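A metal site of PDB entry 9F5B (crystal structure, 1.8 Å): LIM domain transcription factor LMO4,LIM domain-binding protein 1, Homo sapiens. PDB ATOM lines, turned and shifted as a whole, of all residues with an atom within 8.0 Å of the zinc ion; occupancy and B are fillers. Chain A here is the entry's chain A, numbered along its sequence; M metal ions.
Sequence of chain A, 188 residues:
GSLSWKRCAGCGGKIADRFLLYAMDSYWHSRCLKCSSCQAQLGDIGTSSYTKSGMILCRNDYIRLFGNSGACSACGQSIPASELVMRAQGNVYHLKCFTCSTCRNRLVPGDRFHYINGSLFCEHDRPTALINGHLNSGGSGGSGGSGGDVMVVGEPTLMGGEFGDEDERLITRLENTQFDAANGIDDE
A ring nitrogen (ND1) of His 29 is bound to the zinc ion, at 2.2 Å. SG of Cys 32 is bound to the zinc ion (2.2 Å). The zinc ion is bound by SG of Cys 8, 2.3 Å away. The zinc ion is bound by SG of Cys 11. The zinc ion has four donor atoms within binding distance.
The backbone carbonyl oxygen (O) of Lys 14 sits at hydrogen-bond distance from a ring nitrogen (NE2) of His 29 (3.4 Å). The guanidinium group of Arg 31 sits close to the side-chain sulfur of Cys 32 (3.8 Å). The side-chain sulfur (SG) of Cys 8 lies close to the backbone NH (N) of Gly 10 (3.2 Å). N of Cys 8 is in hydrogen-bond range of O of Gly 13, 2.8 Å away. The side-chain sulfur of Cys 11 lies close to the backbone NH of Gly 13 (3.4 Å).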
ATOM      1  N   ARG A   7      14.496 -22.082   5.314  1.00  0.00           N
ATOM      2  CA  ARG A   7      13.438 -21.689   6.220  1.00  0.00           C
ATOM      3  C   ARG A   7      12.495 -22.861   6.467  1.00  0.00           C
ATOM      4  O   ARG A   7      12.221 -23.666   5.577  1.00  0.00           O
ATOM      5  CB  ARG A   7      12.627 -20.512   5.686  1.00  0.00           C
ATOM      6  CG  ARG A   7      13.446 -19.220   5.577  1.00  0.00           C
ATOM      7  CD  ARG A   7      12.539 -18.005   5.809  1.00  0.00           C
ATOM      8  NE  ARG A   7      13.355 -16.852   6.184  1.00  0.00           N
ATOM      9  CZ  ARG A   7      13.283 -16.243   7.366  1.00  0.00           C
ATOM     10  NH1 ARG A   7      12.567 -16.746   8.345  1.00  0.00           N
ATOM     11  NH2 ARG A   7      13.972 -15.143   7.610  1.00  0.00           N
ATOM     12  N   CYS A   8      11.980 -22.917   7.700  1.00  0.00           N
ATOM     13  CA  CYS A   8      11.087 -23.994   8.091  1.00  0.00           C
ATOM     14  C   CYS A   8       9.666 -23.658   7.622  1.00  0.00           C
ATOM     15  O   CYS A   8       9.164 -22.563   7.893  1.00  0.00           O
ATOM     16  CB  CYS A   8      11.124 -24.106   9.595  1.00  0.00           C
ATOM     17  SG  CYS A   8       9.990 -25.321  10.253  1.00  0.00           S
ATOM     18  N   ALA A   9       9.031 -24.602   6.917  1.00  0.00           N
ATOM     19  CA  ALA A   9       7.642 -24.393   6.498  1.00  0.00           C
ATOM     20  C   ALA A   9       6.686 -24.428   7.673  1.00  0.00           C
ATOM     21  O   ALA A   9       5.551 -23.964   7.551  1.00  0.00           O
ATOM     22  CB  ALA A   9       7.229 -25.440   5.464  1.00  0.00           C
ATOM     23  N   GLY A  10       7.109 -24.976   8.813  1.00  0.00           N
ATOM     24  CA  GLY A  10       6.203 -25.064   9.953  1.00  0.00           C
ATOM     25  C   GLY A  10       6.122 -23.761  10.754  1.00  0.00           C
ATOM     26  O   GLY A  10       5.027 -23.366  11.135  1.00  0.00           O
ATOM     27  N   CYS A  11       7.269 -23.091  10.945  1.00  0.00           N
ATOM     28  CA  CYS A  11       7.336 -21.911  11.799  1.00  0.00           C
ATOM     29  C   CYS A  11       7.829 -20.631  11.099  1.00  0.00           C
ATOM     30  O   CYS A  11       7.758 -19.560  11.702  1.00  0.00           O
ATOM     31  CB  CYS A  11       8.185 -22.163  13.055  1.00  0.00           C
ATOM     32  SG  CYS A  11       9.971 -22.324  12.738  1.00  0.00           S
ATOM     33  N   GLY A  12       8.330 -20.738   9.862  1.00  0.00           N
ATOM     34  CA  GLY A  12       8.893 -19.613   9.119  1.00  0.00           C
ATOM     35  C   GLY A  12      10.325 -19.240   9.504  1.00  0.00           C
ATOM     36  O   GLY A  12      10.904 -18.340   8.903  1.00  0.00           O
ATOM     37  N   GLY A  13      10.906 -19.867  10.522  1.00  0.00           N
ATOM     38  CA  GLY A  13      12.234 -19.485  10.976  1.00  0.00           C
ATOM     39  C   GLY A  13      13.361 -20.156  10.197  1.00  0.00           C
ATOM     40  O   GLY A  13      13.185 -21.203   9.575  1.00  0.00           O
ATOM     41  N   LYS A  14      14.547 -19.549  10.223  1.00  0.00           N
ATOM     42  CA  LYS A  14      15.721 -20.188   9.646  1.00  0.00           C
ATOM     43  C   LYS A  14      16.029 -21.439  10.461  1.00  0.00           C
ATOM     44  O   LYS A  14      15.828 -21.484  11.684  1.00  0.00           O
ATOM     45  CB  LYS A  14      16.924 -19.249   9.664  1.00  0.00           C
ATOM     46  CG  LYS A  14      16.747 -18.065   8.685  1.00  0.00           C
ATOM     47  CD  LYS A  14      18.070 -17.304   8.562  1.00  0.00           C
ATOM     48  CE  LYS A  14      17.936 -15.845   8.176  1.00  0.00           C
ATOM     49  NZ  LYS A  14      19.221 -15.140   8.169  1.00  0.00           N
ATOM     50  N   ILE A  15      16.524 -22.463   9.778  1.00  0.00           N
ATOM     51  CA  ILE A  15      16.858 -23.718  10.430  1.00  0.00           C
ATOM     52  C   ILE A  15      18.374 -23.779  10.606  1.00  0.00           C
ATOM     53  O   ILE A  15      19.116 -24.008   9.632  1.00  0.00           O
ATOM     54  CB  ILE A  15      16.357 -24.940   9.641  1.00  0.00           C
ATOM     55  CG1 ILE A  15      14.851 -24.903   9.427  1.00  0.00           C
ATOM     56  CG2 ILE A  15      16.717 -26.223  10.402  1.00  0.00           C
ATOM     57  CD1 ILE A  15      14.372 -25.853   8.317  1.00  0.00           C
ATOM     58  N   ASP A  17      19.632 -25.924  13.004  1.00  0.00           N
ATOM     59  CA  ASP A  17      19.842 -27.218  13.625  1.00  0.00           C
ATOM     60  C   ASP A  17      20.763 -28.108  12.800  1.00  0.00           C
ATOM     61  O   ASP A  17      20.745 -28.070  11.567  1.00  0.00           O
ATOM     62  CB  ASP A  17      18.532 -27.979  13.727  1.00  0.00           C
ATOM     63  CG  ASP A  17      17.507 -27.308  14.587  1.00  0.00           C
ATOM     64  OD1 ASP A  17      17.825 -26.227  15.107  1.00  0.00           O
ATOM     65  OD2 ASP A  17      16.419 -27.925  14.717  1.00  0.00           O
ATOM     66  N   TYR A  27      11.590 -27.681   3.812  1.00  0.00           N
ATOM     67  CA  TYR A  27      12.463 -28.018   4.942  1.00  0.00           C
ATOM     68  C   TYR A  27      11.738 -27.719   6.244  1.00  0.00           C
ATOM     69  O   TYR A  27      10.882 -26.836   6.294  1.00  0.00           O
ATOM     70  CB  TYR A  27      13.749 -27.185   4.888  1.00  0.00           C
ATOM     71  CG  TYR A  27      14.545 -27.490   3.637  1.00  0.00           C
ATOM     72  CD1 TYR A  27      14.312 -26.774   2.465  1.00  0.00           C
ATOM     73  CD2 TYR A  27      15.499 -28.499   3.622  1.00  0.00           C
ATOM     74  CE1 TYR A  27      15.025 -27.069   1.307  1.00  0.00           C
ATOM     75  CE2 TYR A  27      16.228 -28.781   2.469  1.00  0.00           C
ATOM     76  CZ  TYR A  27      15.977 -28.075   1.305  1.00  0.00           C
ATOM     77  OH  TYR A  27      16.693 -28.346   0.163  1.00  0.00           O
ATOM     78  N   TRP A  28      12.107 -28.447   7.314  1.00  0.00           N
ATOM     79  CA  TRP A  28      11.439 -28.337   8.609  1.00  0.00           C
ATOM     80  C   TRP A  28      12.417 -28.534   9.764  1.00  0.00           C
ATOM     81  O   TRP A  28      13.216 -29.488   9.716  1.00  0.00           O
ATOM     82  CB  TRP A  28      10.380 -29.440   8.767  1.00  0.00           C
ATOM     83  CG  TRP A  28       9.407 -29.562   7.633  1.00  0.00           C
ATOM     84  CD1 TRP A  28       9.632 -30.140   6.401  1.00  0.00           C
ATOM     85  CD2 TRP A  28       8.036 -29.146   7.645  1.00  0.00           C
ATOM     86  NE1 TRP A  28       8.490 -30.078   5.650  1.00  0.00           N
ATOM     87  CE2 TRP A  28       7.512 -29.457   6.380  1.00  0.00           C
ATOM     88  CE3 TRP A  28       7.220 -28.513   8.582  1.00  0.00           C
ATOM     89  CZ2 TRP A  28       6.180 -29.180   6.032  1.00  0.00           C
ATOM     90  CZ3 TRP A  28       5.900 -28.244   8.236  1.00  0.00           C
ATOM     91  CH2 TRP A  28       5.393 -28.554   6.972  1.00  0.00           C
ATOM     92  N   HIS A  29      12.282 -27.748  10.831  1.00  0.00           N
ATOM     93  CA  HIS A  29      12.744 -28.264  12.128  1.00  0.00           C
ATOM     94  C   HIS A  29      11.944 -29.519  12.419  1.00  0.00           C
ATOM     95  O   HIS A  29      10.750 -29.573  12.164  1.00  0.00           O
ATOM     96  CB  HIS A  29      12.460 -27.274  13.278  1.00  0.00           C
ATOM     97  CG  HIS A  29      13.147 -25.953  13.152  1.00  0.00           C
ATOM     98  ND1 HIS A  29      12.484 -24.809  12.782  1.00  0.00           N
ATOM     99  CD2 HIS A  29      14.417 -25.576  13.457  1.00  0.00           C
ATOM    100  CE1 HIS A  29      13.311 -23.758  12.839  1.00  0.00           C
ATOM    101  NE2 HIS A  29      14.502 -24.211  13.246  1.00  0.00           N
ATOM    102  N   SER A  30      12.590 -30.552  12.967  1.00  0.00           N
ATOM    103  CA  SER A  30      11.827 -31.767  13.210  1.00  0.00           C
ATOM    104  C   SER A  30      10.630 -31.480  14.146  1.00  0.00           C
ATOM    105  O   SER A  30       9.528 -31.989  13.927  1.00  0.00           O
ATOM    106  CB  SER A  30      12.705 -32.876  13.772  1.00  0.00           C
ATOM    107  OG  SER A  30      11.901 -34.022  13.940  1.00  0.00           O
ATOM    108  N   ARG A  31      10.828 -30.664  15.172  1.00  0.00           N
ATOM    109  CA  ARG A  31       9.752 -30.340  16.105  1.00  0.00           C
ATOM    110  C   ARG A  31       8.574 -29.628  15.415  1.00  0.00           C
ATOM    111  O   ARG A  31       7.463 -29.619  15.944  1.00  0.00           O
ATOM    112  CB  ARG A  31      10.247 -29.435  17.240  1.00  0.00           C
ATOM    113  CG  ARG A  31      10.878 -28.137  16.752  1.00  0.00           C
ATOM    114  CD  ARG A  31      11.520 -27.326  17.876  1.00  0.00           C
ATOM    115  NE  ARG A  31      12.407 -26.294  17.304  1.00  0.00           N
ATOM    116  CZ  ARG A  31      12.018 -25.089  16.903  1.00  0.00           C
ATOM    117  NH1 ARG A  31      10.759 -24.699  17.032  1.00  0.00           N
ATOM    118  NH2 ARG A  31      12.904 -24.260  16.380  1.00  0.00           N
ATOM    119  N   CYS A  32       8.797 -29.050  14.232  1.00  0.00           N
ATOM    120  CA  CYS A  32       7.756 -28.298  13.553  1.00  0.00           C
ATOM    121  C   CYS A  32       6.946 -29.144  12.573  1.00  0.00           C
ATOM    122  O   CYS A  32       5.963 -28.638  12.014  1.00  0.00           O
ATOM    123  CB  CYS A  32       8.355 -27.127  12.790  1.00  0.00           C
ATOM    124  SG  CYS A  32       9.084 -25.900  13.889  1.00  0.00           S
ATOM    125  N   LEU A  33       7.352 -30.382  12.294  1.00  0.00           N
ATOM    126  CA  LEU A  33       6.587 -31.236  11.393  1.00  0.00           C
ATOM    127  C   LEU A  33       5.786 -32.216  12.243  1.00  0.00           C
ATOM    128  O   LEU A  33       6.308 -33.250  12.687  1.00  0.00           O
ATOM    129  CB  LEU A  33       7.508 -31.927  10.397  1.00  0.00           C
ATOM    130  CG  LEU A  33       6.793 -32.854   9.406  1.00  0.00           C
ATOM    131  CD1 LEU A  33       5.718 -32.109   8.588  1.00  0.00           C
ATOM    132  CD2 LEU A  33       7.770 -33.572   8.501  1.00  0.00           C
HETATM  133 ZN    ZN M   1      10.286 -24.641  12.481  1.00  0.00          ZN
